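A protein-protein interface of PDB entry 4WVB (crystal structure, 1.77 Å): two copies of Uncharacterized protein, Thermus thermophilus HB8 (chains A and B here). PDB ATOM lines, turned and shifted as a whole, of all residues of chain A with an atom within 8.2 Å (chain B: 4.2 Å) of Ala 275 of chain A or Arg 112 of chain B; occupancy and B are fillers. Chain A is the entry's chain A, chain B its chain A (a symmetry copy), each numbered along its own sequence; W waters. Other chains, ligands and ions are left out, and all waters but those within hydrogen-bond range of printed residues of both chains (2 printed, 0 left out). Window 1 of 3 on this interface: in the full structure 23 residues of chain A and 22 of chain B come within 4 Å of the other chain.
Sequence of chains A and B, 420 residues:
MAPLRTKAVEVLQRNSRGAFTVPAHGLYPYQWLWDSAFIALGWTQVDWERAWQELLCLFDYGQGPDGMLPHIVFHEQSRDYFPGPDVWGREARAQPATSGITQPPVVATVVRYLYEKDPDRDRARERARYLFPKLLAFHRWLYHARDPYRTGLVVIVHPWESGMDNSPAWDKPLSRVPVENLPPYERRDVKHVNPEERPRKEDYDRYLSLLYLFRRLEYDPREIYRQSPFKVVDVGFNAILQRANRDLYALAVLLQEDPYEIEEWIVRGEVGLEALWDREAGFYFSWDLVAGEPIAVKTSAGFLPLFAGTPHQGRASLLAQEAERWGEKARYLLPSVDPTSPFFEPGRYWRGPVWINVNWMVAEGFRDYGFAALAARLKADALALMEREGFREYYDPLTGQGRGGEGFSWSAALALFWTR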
ATOM      1  N   THR A 151       8.221  15.037  20.283  1.00  0.00           N
ATOM      2  CA  THR A 151       7.497  16.204  20.783  1.00  0.00           C
ATOM      3  C   THR A 151       6.865  17.044  19.673  1.00  0.00           C
ATOM      4  O   THR A 151       5.903  17.784  19.913  1.00  0.00           O
ATOM      5  CB  THR A 151       8.409  17.147  21.609  1.00  0.00           C
ATOM      6  OG1 THR A 151       9.395  17.786  20.770  1.00  0.00           O
ATOM      7  CG2 THR A 151       9.082  16.373  22.729  1.00  0.00           C
ATOM      8  N   LEU A 153       8.939  19.210  18.176  1.00  0.00           N
ATOM      9  CA  LEU A 153       9.931  20.247  18.129  1.00  0.00           C
ATOM     10  C   LEU A 153      11.336  19.663  18.109  1.00  0.00           C
ATOM     11  O   LEU A 153      11.598  18.687  18.824  1.00  0.00           O
ATOM     12  CB  LEU A 153       9.786  21.141  19.370  1.00  0.00           C
ATOM     13  CG  LEU A 153       8.546  22.019  19.422  1.00  0.00           C
ATOM     14  CD1 LEU A 153       8.306  22.505  20.851  1.00  0.00           C
ATOM     15  CD2 LEU A 153       8.743  23.188  18.453  1.00  0.00           C
ATOM     16  N   VAL A 233      15.330  24.647  21.828  1.00  0.00           N
ATOM     17  CA  VAL A 233      14.300  24.671  20.801  1.00  0.00           C
ATOM     18  C   VAL A 233      14.247  26.081  20.192  1.00  0.00           C
ATOM     19  O   VAL A 233      13.695  27.008  20.812  1.00  0.00           O
ATOM     20  CB  VAL A 233      12.947  24.317  21.412  1.00  0.00           C
ATOM     21  CG1 VAL A 233      11.828  24.472  20.411  1.00  0.00           C
ATOM     22  CG2 VAL A 233      12.987  22.901  21.973  1.00  0.00           C
ATOM     23  N   ARG A 268       2.355  16.989  14.556  1.00  0.00           N
ATOM     24  CA  ARG A 268       3.099  17.252  15.791  1.00  0.00           C
ATOM     25  C   ARG A 268       3.723  18.655  15.814  1.00  0.00           C
ATOM     26  O   ARG A 268       3.760  19.301  16.860  1.00  0.00           O
ATOM     27  CB  ARG A 268       4.180  16.180  16.045  1.00  0.00           C
ATOM     28  CG  ARG A 268       3.617  14.786  16.283  1.00  0.00           C
ATOM     29  CD  ARG A 268       4.636  13.916  17.009  1.00  0.00           C
ATOM     30  NE  ARG A 268       5.832  13.666  16.208  1.00  0.00           N
ATOM     31  CZ  ARG A 268       6.109  12.529  15.560  1.00  0.00           C
ATOM     32  NH1 ARG A 268       5.278  11.486  15.609  1.00  0.00           N
ATOM     33  NH2 ARG A 268       7.245  12.443  14.863  1.00  0.00           N
ATOM     34  N   GLY A 269       4.203  19.097  14.652  1.00  0.00           N
ATOM     35  CA  GLY A 269       4.914  20.347  14.534  1.00  0.00           C
ATOM     36  C   GLY A 269       3.990  21.530  14.689  1.00  0.00           C
ATOM     37  O   GLY A 269       4.415  22.586  15.143  1.00  0.00           O
ATOM     38  N   GLU A 270       2.718  21.351  14.354  1.00  0.00           N
ATOM     39  CA  GLU A 270       1.732  22.419  14.502  1.00  0.00           C
ATOM     40  C   GLU A 270       1.466  22.670  15.983  1.00  0.00           C
ATOM     41  O   GLU A 270       1.359  23.824  16.438  1.00  0.00           O
ATOM     42  CB  GLU A 270       0.474  22.009  13.753  1.00  0.00           C
ATOM     43  CG  GLU A 270      -0.477  23.109  13.448  1.00  0.00           C
ATOM     44  CD  GLU A 270      -0.125  23.882  12.195  1.00  0.00           C
ATOM     45  OE1 GLU A 270       0.862  23.573  11.465  1.00  0.00           O
ATOM     46  OE2 GLU A 270      -0.872  24.837  11.959  1.00  0.00           O
ATOM     47  N   VAL A 271       1.390  21.586  16.754  1.00  0.00           N
ATOM     48  CA  VAL A 271       1.257  21.672  18.196  1.00  0.00           C
ATOM     49  C   VAL A 271       2.519  22.297  18.798  1.00  0.00           C
ATOM     50  O   VAL A 271       2.447  23.200  19.649  1.00  0.00           O
ATOM     51  CB  VAL A 271       1.012  20.256  18.803  1.00  0.00           C
ATOM     52  CG1 VAL A 271       0.944  20.343  20.310  1.00  0.00           C
ATOM     53  CG2 VAL A 271      -0.275  19.649  18.252  1.00  0.00           C
ATOM     54  N   GLY A 272       3.686  21.817  18.373  1.00  0.00           N
ATOM     55  CA  GLY A 272       4.938  22.264  18.934  1.00  0.00           C
ATOM     56  C   GLY A 272       5.199  23.748  18.710  1.00  0.00           C
ATOM     57  O   GLY A 272       5.500  24.492  19.645  1.00  0.00           O
ATOM     58  N   LEU A 273       5.079  24.185  17.471  1.00  0.00           N
ATOM     59  CA  LEU A 273       5.458  25.574  17.167  1.00  0.00           C
ATOM     60  C   LEU A 273       4.527  26.541  17.891  1.00  0.00           C
ATOM     61  O   LEU A 273       4.990  27.575  18.456  1.00  0.00           O
ATOM     62  CB  LEU A 273       5.453  25.825  15.665  1.00  0.00           C
ATOM     63  CG  LEU A 273       6.222  27.086  15.248  1.00  0.00           C
ATOM     64  CD1 LEU A 273       7.713  26.939  15.509  1.00  0.00           C
ATOM     65  CD2 LEU A 273       5.957  27.382  13.778  1.00  0.00           C
ATOM     66  N   GLU A 274       3.236  26.230  17.925  1.00  0.00           N
ATOM     67  CA  GLU A 274       2.305  27.138  18.645  1.00  0.00           C
ATOM     68  C   GLU A 274       2.523  27.179  20.146  1.00  0.00           C
ATOM     69  O   GLU A 274       2.224  28.181  20.806  1.00  0.00           O
ATOM     70  CB  GLU A 274       0.844  26.845  18.309  1.00  0.00           C
ATOM     71  CG  GLU A 274       0.531  27.251  16.880  1.00  0.00           C
ATOM     72  CD  GLU A 274       0.658  28.762  16.715  1.00  0.00           C
ATOM     73  OE1 GLU A 274      -0.162  29.472  17.318  1.00  0.00           O
ATOM     74  OE2 GLU A 274       1.622  29.194  16.060  1.00  0.00           O
ATOM     75  N   ALA A 275       3.078  26.097  20.698  1.00  0.00           N
ATOM     76  CA  ALA A 275       3.399  26.088  22.123  1.00  0.00           C
ATOM     77  C   ALA A 275       4.409  27.188  22.507  1.00  0.00           C
ATOM     78  O   ALA A 275       4.451  27.582  23.664  1.00  0.00           O
ATOM     79  CB  ALA A 275       3.942  24.729  22.530  1.00  0.00           C
ATOM     80  N   LEU A 276       5.220  27.628  21.548  1.00  0.00           N
ATOM     81  CA  LEU A 276       6.284  28.603  21.816  1.00  0.00           C
ATOM     82  C   LEU A 276       5.743  30.019  22.021  1.00  0.00           C
ATOM     83  O   LEU A 276       6.501  30.911  22.417  1.00  0.00           O
ATOM     84  CB  LEU A 276       7.350  28.590  20.719  1.00  0.00           C
ATOM     85  CG  LEU A 276       8.026  27.216  20.455  1.00  0.00           C
ATOM     86  CD1 LEU A 276       9.093  27.395  19.416  1.00  0.00           C
ATOM     87  CD2 LEU A 276       8.641  26.615  21.715  1.00  0.00           C
ATOM     88  N   TRP A 277       4.456  30.224  21.755  1.00  0.00           N
ATOM     89  CA  TRP A 277       3.857  31.561  21.950  1.00  0.00           C
ATOM     90  C   TRP A 277       3.723  31.864  23.438  1.00  0.00           C
ATOM     91  O   TRP A 277       3.179  31.075  24.211  1.00  0.00           O
ATOM     92  CB  TRP A 277       2.486  31.615  21.304  1.00  0.00           C
ATOM     93  CG  TRP A 277       1.771  32.889  21.547  1.00  0.00           C
ATOM     94  CD1 TRP A 277       0.799  33.142  22.466  1.00  0.00           C
ATOM     95  CD2 TRP A 277       1.979  34.111  20.827  1.00  0.00           C
ATOM     96  NE1 TRP A 277       0.376  34.462  22.370  1.00  0.00           N
ATOM     97  CE2 TRP A 277       1.077  35.073  21.358  1.00  0.00           C
ATOM     98  CE3 TRP A 277       2.846  34.484  19.794  1.00  0.00           C
ATOM     99  CZ2 TRP A 277       1.029  36.398  20.893  1.00  0.00           C
ATOM    100  CZ3 TRP A 277       2.784  35.805  19.297  1.00  0.00           C
ATOM    101  CH2 TRP A 277       1.872  36.741  19.848  1.00  0.00           C
ATOM    102  N   ASP A 278       4.218  33.029  23.838  1.00  0.00           N
ATOM    103  CA  ASP A 278       4.100  33.479  25.196  1.00  0.00           C
ATOM    104  C   ASP A 278       3.032  34.575  25.231  1.00  0.00           C
ATOM    105  O   ASP A 278       3.214  35.639  24.633  1.00  0.00           O
ATOM    106  CB  ASP A 278       5.421  34.056  25.693  1.00  0.00           C
ATOM    107  CG  ASP A 278       5.378  34.365  27.170  1.00  0.00           C
ATOM    108  OD1 ASP A 278       5.620  33.441  27.979  1.00  0.00           O
ATOM    109  OD2 ASP A 278       5.036  35.500  27.527  1.00  0.00           O
ATOM    110  N   ARG A 279       1.917  34.291  25.888  1.00  0.00           N
ATOM    111  CA  ARG A 279       0.758  35.200  25.876  1.00  0.00           C
ATOM    112  C   ARG A 279       1.062  36.490  26.622  1.00  0.00           C
ATOM    113  O   ARG A 279       0.585  37.554  26.221  1.00  0.00           O
ATOM    114  CB  ARG A 279      -0.481  34.549  26.483  1.00  0.00           C
ATOM    115  CG  ARG A 279      -1.112  33.473  25.600  1.00  0.00           C
ATOM    116  CD  ARG A 279      -2.152  32.692  26.381  1.00  0.00           C
ATOM    117  NE  ARG A 279      -3.052  31.863  25.587  1.00  0.00           N
ATOM    118  CZ  ARG A 279      -2.810  30.587  25.258  1.00  0.00           C
ATOM    119  NH1 ARG A 279      -1.656  30.008  25.599  1.00  0.00           N
ATOM    120  NH2 ARG A 279      -3.714  29.898  24.561  1.00  0.00           N
ATOM    121  N   PHE A 283       4.577  37.257  22.096  1.00  0.00           N
ATOM    122  CA  PHE A 283       5.634  36.947  21.136  1.00  0.00           C
ATOM    123  C   PHE A 283       5.938  35.466  21.214  1.00  0.00           C
ATOM    124  O   PHE A 283       5.571  34.819  22.197  1.00  0.00           O
ATOM    125  CB  PHE A 283       6.896  37.750  21.453  1.00  0.00           C
ATOM    126  CG  PHE A 283       7.721  38.101  20.252  1.00  0.00           C
ATOM    127  CD1 PHE A 283       7.252  39.002  19.303  1.00  0.00           C
ATOM    128  CD2 PHE A 283       8.977  37.576  20.092  1.00  0.00           C
ATOM    129  CE1 PHE A 283       7.988  39.311  18.191  1.00  0.00           C
ATOM    130  CE2 PHE A 283       9.752  37.899  18.994  1.00  0.00           C
ATOM    131  CZ  PHE A 283       9.264  38.765  18.023  1.00  0.00           C
ATOM    132  N   TYR A 284       6.630  34.973  20.198  1.00  0.00           N
ATOM    133  CA  TYR A 284       7.161  33.591  20.196  1.00  0.00           C
ATOM    134  C   TYR A 284       8.617  33.589  20.681  1.00  0.00           C
ATOM    135  O   TYR A 284       9.450  34.321  20.145  1.00  0.00           O
ATOM    136  CB  TYR A 284       7.145  32.984  18.799  1.00  0.00           C
ATOM    137  CG  TYR A 284       5.809  32.665  18.179  1.00  0.00           C
ATOM    138  CD1 TYR A 284       5.217  31.427  18.368  1.00  0.00           C
ATOM    139  CD2 TYR A 284       5.161  33.577  17.336  1.00  0.00           C
ATOM    140  CE1 TYR A 284       4.028  31.110  17.761  1.00  0.00           C
ATOM    141  CE2 TYR A 284       3.957  33.269  16.742  1.00  0.00           C
ATOM    142  CZ  TYR A 284       3.391  32.035  16.963  1.00  0.00           C
ATOM    143  OH  TYR A 284       2.208  31.708  16.366  1.00  0.00           O
ATOM    144  N   PHE A 285       8.912  32.715  21.647  1.00  0.00           N
ATOM    145  CA  PHE A 285      10.242  32.589  22.223  1.00  0.00           C
ATOM    146  C   PHE A 285      10.827  31.208  21.901  1.00  0.00           C
ATOM    147  O   PHE A 285      10.094  30.216  21.818  1.00  0.00           O
ATOM    148  CB  PHE A 285      10.184  32.734  23.744  1.00  0.00           C
ATOM    149  CG  PHE A 285       9.879  34.132  24.242  1.00  0.00           C
ATOM    150  CD1 PHE A 285      10.452  35.255  23.649  1.00  0.00           C
ATOM    151  CD2 PHE A 285       9.054  34.300  25.345  1.00  0.00           C
ATOM    152  CE1 PHE A 285      10.165  36.526  24.138  1.00  0.00           C
ATOM    153  CE2 PHE A 285       8.788  35.557  25.854  1.00  0.00           C
ATOM    154  CZ  PHE A 285       9.342  36.674  25.236  1.00  0.00           C
ATOM    155  N   TRP A 287      13.116  28.092  23.377  1.00  0.00           N
ATOM    156  CA  TRP A 287      13.128  27.494  24.696  1.00  0.00           C
ATOM    157  C   TRP A 287      14.478  26.853  24.993  1.00  0.00           C
ATOM    158  O   TRP A 287      15.094  26.226  24.112  1.00  0.00           O
ATOM    159  CB  TRP A 287      12.024  26.438  24.850  1.00  0.00           C
ATOM    160  CG  TRP A 287      10.633  26.973  24.907  1.00  0.00           C
ATOM    161  CD1 TRP A 287      10.241  28.291  24.883  1.00  0.00           C
ATOM    162  CD2 TRP A 287       9.445  26.212  25.056  1.00  0.00           C
ATOM    163  NE1 TRP A 287       8.892  28.382  25.000  1.00  0.00           N
ATOM    164  CE2 TRP A 287       8.375  27.118  25.118  1.00  0.00           C
ATOM    165  CE3 TRP A 287       9.173  24.835  25.128  1.00  0.00           C
ATOM    166  CZ2 TRP A 287       7.068  26.706  25.260  1.00  0.00           C
ATOM    167  CZ3 TRP A 287       7.855  24.426  25.259  1.00  0.00           C
ATOM    168  CH2 TRP A 287       6.821  25.366  25.328  1.00  0.00           C
ATOM    169  N   PRO A 294      11.444  29.032  28.852  1.00  0.00           N
ATOM    170  CA  PRO A 294      11.475  29.930  27.704  1.00  0.00           C
ATOM    171  C   PRO A 294      12.597  30.961  27.821  1.00  0.00           C
ATOM    172  O   PRO A 294      12.932  31.371  28.931  1.00  0.00           O
ATOM    173  CB  PRO A 294      10.107  30.609  27.759  1.00  0.00           C
ATOM    174  CG  PRO A 294       9.236  29.658  28.487  1.00  0.00           C
ATOM    175  CD  PRO A 294      10.148  29.097  29.550  1.00  0.00           C
ATOM    176  N   THR A 310       1.366  28.750  11.086  1.00  0.00           N
ATOM    177  CA  THR A 310       0.729  28.185  12.282  1.00  0.00           C
ATOM    178  C   THR A 310      -0.151  29.106  13.154  1.00  0.00           C
ATOM    179  O   THR A 310      -1.150  28.643  13.697  1.00  0.00           O
ATOM    180  CB  THR A 310       1.773  27.480  13.191  1.00  0.00           C
ATOM    181  OG1 THR A 310       2.673  28.434  13.759  1.00  0.00           O
ATOM    182  CG2 THR A 310       2.559  26.454  12.386  1.00  0.00           C
ATOM    183  N   ARG A 315      -3.252  36.232  16.595  1.00  0.00           N
ATOM    184  CA  ARG A 315      -1.868  36.121  16.946  1.00  0.00           C
ATOM    185  C   ARG A 315      -0.946  36.823  15.915  1.00  0.00           C
ATOM    186  O   ARG A 315      -0.019  37.555  16.288  1.00  0.00           O
ATOM    187  CB  ARG A 315      -1.532  34.639  17.058  1.00  0.00           C
ATOM    188  CG  ARG A 315      -0.212  34.344  17.688  1.00  0.00           C
ATOM    189  CD  ARG A 315      -0.221  32.922  18.281  1.00  0.00           C
ATOM    190  NE  ARG A 315      -1.041  32.848  19.477  1.00  0.00           N
ATOM    191  CZ  ARG A 315      -1.194  31.769  20.236  1.00  0.00           C
ATOM    192  NH1 ARG A 315      -0.549  30.636  19.951  1.00  0.00           N
ATOM    193  NH2 ARG A 315      -1.958  31.851  21.328  1.00  0.00           N
ATOM    194  N   ALA B 108      -3.794  22.454  35.179  1.00  0.00           N
ATOM    195  CA  ALA B 108      -2.533  22.370  34.464  1.00  0.00           C
ATOM    196  C   ALA B 108      -2.103  23.743  33.954  1.00  0.00           C
ATOM    197  O   ALA B 108      -0.930  24.063  33.941  1.00  0.00           O
ATOM    198  CB  ALA B 108      -2.607  21.363  33.305  1.00  0.00           C
ATOM    199  N   THR B 109      -3.074  24.556  33.561  1.00  0.00           N
ATOM    200  CA  THR B 109      -2.810  25.923  33.125  1.00  0.00           C
ATOM    201  C   THR B 109      -2.174  26.763  34.271  1.00  0.00           C
ATOM    202  O   THR B 109      -1.209  27.514  34.052  1.00  0.00           O
ATOM    203  CB  THR B 109      -4.124  26.551  32.625  1.00  0.00           C
ATOM    204  OG1 THR B 109      -4.561  25.882  31.442  1.00  0.00           O
ATOM    205  CG2 THR B 109      -3.973  28.051  32.320  1.00  0.00           C
ATOM    206  N   VAL B 110      -2.680  26.596  35.482  1.00  0.00           N
ATOM    207  CA  VAL B 110      -2.106  27.241  36.665  1.00  0.00           C
ATOM    208  C   VAL B 110      -0.697  26.742  36.955  1.00  0.00           C
ATOM    209  O   VAL B 110       0.227  27.542  37.197  1.00  0.00           O
ATOM    210  CB  VAL B 110      -3.029  27.112  37.881  1.00  0.00           C
ATOM    211  CG1 VAL B 110      -2.393  27.704  39.139  1.00  0.00           C
ATOM    212  CG2 VAL B 110      -4.379  27.768  37.575  1.00  0.00           C
ATOM    213  N   VAL B 111      -0.514  25.419  36.934  1.00  0.00           N
ATOM    214  CA  VAL B 111       0.797  24.864  37.233  1.00  0.00           C
ATOM    215  C   VAL B 111       1.831  25.343  36.218  1.00  0.00           C
ATOM    216  O   VAL B 111       2.955  25.626  36.599  1.00  0.00           O
ATOM    217  CB  VAL B 111       0.771  23.326  37.259  1.00  0.00           C
ATOM    218  CG1 VAL B 111       2.179  22.789  37.370  1.00  0.00           C
ATOM    219  CG2 VAL B 111      -0.062  22.843  38.432  1.00  0.00           C
ATOM    220  N   ARG B 112       1.467  25.434  34.936  1.00  0.00           N
ATOM    221  CA  ARG B 112       2.386  25.985  33.931  1.00  0.00           C
ATOM    222  C   ARG B 112       2.817  27.417  34.299  1.00  0.00           C
ATOM    223  O   ARG B 112       4.006  27.759  34.235  1.00  0.00           O
ATOM    224  CB  ARG B 112       1.782  26.004  32.538  1.00  0.00           C
ATOM    225  CG  ARG B 112       2.764  26.510  31.488  1.00  0.00           C
ATOM    226  CD  ARG B 112       2.172  26.607  30.119  1.00  0.00           C
ATOM    227  NE  ARG B 112       3.121  27.224  29.198  1.00  0.00           N
ATOM    228  CZ  ARG B 112       2.895  27.465  27.925  1.00  0.00           C
ATOM    229  NH1 ARG B 112       1.744  27.148  27.352  1.00  0.00           N
ATOM    230  NH2 ARG B 112       3.851  28.021  27.203  1.00  0.00           N
ATOM    231  N   TYR B 113       1.845  28.240  34.671  1.00  0.00           N
ATOM    232  CA  TYR B 113       2.156  29.613  35.115  1.00  0.00           C
ATOM    233  C   TYR B 113       3.115  29.605  36.310  1.00  0.00           C
ATOM    234  O   TYR B 113       4.159  30.273  36.285  1.00  0.00           O
ATOM    235  CB  TYR B 113       0.899  30.403  35.482  1.00  0.00           C
ATOM    236  CG  TYR B 113       1.310  31.809  35.901  1.00  0.00           C
ATOM    237  CD1 TYR B 113       1.549  32.796  34.952  1.00  0.00           C
ATOM    238  CD2 TYR B 113       1.545  32.107  37.234  1.00  0.00           C
ATOM    239  CE1 TYR B 113       1.971  34.076  35.343  1.00  0.00           C
ATOM    240  CE2 TYR B 113       1.974  33.372  37.621  1.00  0.00           C
ATOM    241  CZ  TYR B 113       2.182  34.338  36.673  1.00  0.00           C
ATOM    242  OH  TYR B 113       2.621  35.590  37.093  1.00  0.00           O
ATOM    243  N   LEU B 114       2.795  28.832  37.335  1.00  0.00           N
ATOM    244  CA  LEU B 114       3.658  28.772  38.519  1.00  0.00           C
ATOM    245  C   LEU B 114       5.061  28.309  38.152  1.00  0.00           C
ATOM    246  O   LEU B 114       6.073  28.861  38.624  1.00  0.00           O
ATOM    247  CB  LEU B 114       3.081  27.841  39.586  1.00  0.00           C
ATOM    248  CG  LEU B 114       1.733  28.187  40.192  1.00  0.00           C
ATOM    249  CD1 LEU B 114       1.327  27.127  41.207  1.00  0.00           C
ATOM    250  CD2 LEU B 114       1.777  29.558  40.836  1.00  0.00           C
ATOM    251  N   TYR B 115       5.140  27.284  37.300  1.00  0.00           N
ATOM    252  CA  TYR B 115       6.439  26.814  36.852  1.00  0.00           C
ATOM    253  C   TYR B 115       7.251  27.896  36.120  1.00  0.00           C
ATOM    254  O   TYR B 115       8.433  28.085  36.412  1.00  0.00           O
ATOM    255  CB  TYR B 115       6.298  25.579  35.941  1.00  0.00           C
ATOM    256  CG  TYR B 115       7.632  25.169  35.409  1.00  0.00           C
ATOM    257  CD1 TYR B 115       8.573  24.589  36.261  1.00  0.00           C
ATOM    258  CD2 TYR B 115       7.973  25.353  34.085  1.00  0.00           C
ATOM    259  CE1 TYR B 115       9.832  24.255  35.800  1.00  0.00           C
ATOM    260  CE2 TYR B 115       9.225  24.995  33.611  1.00  0.00           C
ATOM    261  CZ  TYR B 115      10.148  24.440  34.476  1.00  0.00           C
ATOM    262  OH  TYR B 115      11.387  24.084  34.009  1.00  0.00           O
ATOM    263  N   GLU B 116       6.627  28.597  35.187  1.00  0.00           N
ATOM    264  CA  GLU B 116       7.345  29.537  34.323  1.00  0.00           C
ATOM    265  C   GLU B 116       7.775  30.796  35.069  1.00  0.00           C
ATOM    266  O   GLU B 116       8.827  31.383  34.756  1.00  0.00           O
ATOM    267  CB  GLU B 116       6.511  29.898  33.097  1.00  0.00           C
ATOM    268  CG  GLU B 116       6.429  28.720  32.113  1.00  0.00           C
ATOM    269  CD  GLU B 116       5.904  29.120  30.761  1.00  0.00           C
ATOM    270  OE1 GLU B 116       5.832  30.327  30.494  1.00  0.00           O
ATOM    271  OE2 GLU B 116       5.593  28.240  29.940  1.00  0.00           O
ATOM    272  N   ASP B 247      -1.329  23.463  27.772  1.00  0.00           N
ATOM    273  CA  ASP B 247      -0.390  23.911  28.769  1.00  0.00           C
ATOM    274  C   ASP B 247       0.393  22.732  29.371  1.00  0.00           C
ATOM    275  O   ASP B 247       1.555  22.868  29.698  1.00  0.00           O
ATOM    276  CB  ASP B 247      -1.111  24.737  29.832  1.00  0.00           C
ATOM    277  CG  ASP B 247      -1.576  26.074  29.278  1.00  0.00           C
ATOM    278  OD1 ASP B 247      -0.868  26.609  28.397  1.00  0.00           O
ATOM    279  OD2 ASP B 247      -2.618  26.591  29.735  1.00  0.00           O
ATOM    280  N   TYR B 249       1.130  19.989  27.657  1.00  0.00           N
ATOM    281  CA  TYR B 249       2.105  19.732  26.602  1.00  0.00           C
ATOM    282  C   TYR B 249       3.341  20.619  26.759  1.00  0.00           C
ATOM    283  O   TYR B 249       4.472  20.136  26.721  1.00  0.00           O
ATOM    284  CB  TYR B 249       1.463  19.910  25.205  1.00  0.00           C
ATOM    285  CG  TYR B 249       2.499  19.905  24.123  1.00  0.00           C
ATOM    286  CD1 TYR B 249       2.929  18.720  23.550  1.00  0.00           C
ATOM    287  CD2 TYR B 249       3.106  21.107  23.697  1.00  0.00           C
ATOM    288  CE1 TYR B 249       3.925  18.718  22.589  1.00  0.00           C
ATOM    289  CE2 TYR B 249       4.095  21.110  22.738  1.00  0.00           C
ATOM    290  CZ  TYR B 249       4.488  19.912  22.167  1.00  0.00           C
ATOM    291  OH  TYR B 249       5.486  19.934  21.240  1.00  0.00           O
ATOM    292  N   ALA B 250       3.146  21.928  26.934  1.00  0.00           N
ATOM    293  CA  ALA B 250       4.267  22.860  27.076  1.00  0.00           C
ATOM    294  C   ALA B 250       5.127  22.466  28.286  1.00  0.00           C
ATOM    295  O   ALA B 250       6.358  22.414  28.196  1.00  0.00           O
ATOM    296  CB  ALA B 250       3.751  24.289  27.249  1.00  0.00           C
HETATM  297  O   HOH W   1      -1.704  27.059  25.770  1.00  0.00           O
HETATM  298  O   HOH W   2       5.546  30.613  27.591  1.00  0.00           O
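The backbone carbonyl oxygen (O) of Thr 151 of chain A is in hydrogen-bond range of the side-chain hydroxyl (OH) of Tyr 249 of chain B, at 2.6 Å.
N of Leu 153 of chain A lies within hydrogen-bond range of OG1 of Thr 151 of chain A (3.0 Å). O of Trp 287 of chain A is in hydrogen-bond range of N of Val 233 of chain A (2.8 Å). The guanidinium group (NE) of Arg 112 of chain B is in salt-bridge range of the side-chain carboxylate (OE2) of Glu 116 of chain B (2.8 Å). The side-chain carboxylate (OD1) of Asp 247 of chain B lies within salt-bridge range of the guanidinium group (NH1) of Arg 112 of chain B (2.9 Å).
Tyr 249 of chain B touches Leu 153 of chain A. Tyr 249 of chain B touches Gly 272 of chain A. O of Ala 275 of chain A touches NH2 of Arg 112 of chain B, at 3.6 Å. Ala 275 of chain A touches Tyr 249 of chain B (CB to CE2, 3.6 Å). Trp 287 of chain A touches Arg 112 of chain B. Trp 287 of chain A touches Ala 250 of chain B.
Printed residues of chain B within 4 Å of Thr 151 of chain A: Tyr 249. Of the printed residues of chain B, Leu 153 of chain A touches Tyr 249. Glu 270 of chain A touches none of the printed residues of chain B. Ala 275 of chain A touches two residues of chain B. Printed residues of chain B within 4 Å of Trp 287 of chain A: Arg 112 (3.98 Å) and Ala 250 (3.8 Å). Of the printed residues of chain A, Arg 112 of chain B touches Ala 275 (3.6 Å) and Trp 287 (3.98 Å). Asp 247 of chain B touches none of the printed residues of chain A. Of the printed residues of chain A, Tyr 249 of chain B touches Thr 151 (2.6 Å), Leu 153 (3.8 Å), Gly 272 (3.3 Å) and Ala 275 (3.6 Å). Printed residues of chain A within 4 Å of Ala 250 of chain B: Trp 287. The nearest printed residue of chain B that does not touch Ala 275 of chain A is Ala 250 of chain B (4.7 Å). The nearest printed residue of chain A that does not touch Arg 112 of chain B is Trp 277 of chain A (4.3 Å). The nearest printed residue of chain B that does not touch Leu 153 of chain A is Ala 250 of chain B (7.4 Å).
Printed residues of chain A that touch a printed residue of chain B: Thr 151, Leu 153, Gly 272, Ala 275 and Trp 287. Hydrophobic or aromatic side chains of chain A within 4 Å of the printed part of chain B: Leu 153, Ala 275 and Trp 287. Printed residues of chain B that touch a printed residue of chain A: Arg 112, Tyr 249 and Ala 250.
No position is printed for both chains. Of the 7 pairs that touch across the chains among the printed residues, none has its exchanged pair printed and touching as well.
Water W1 bridges OD1 of Asp 247 of chain B and NH1 of Arg 279 of chain A. Water W2 lies within hydrogen-bond range of OD1 of Asp 278 of chain A, OE1 of Glu 116 of chain B and NH2 of Arg 112 of chain B.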
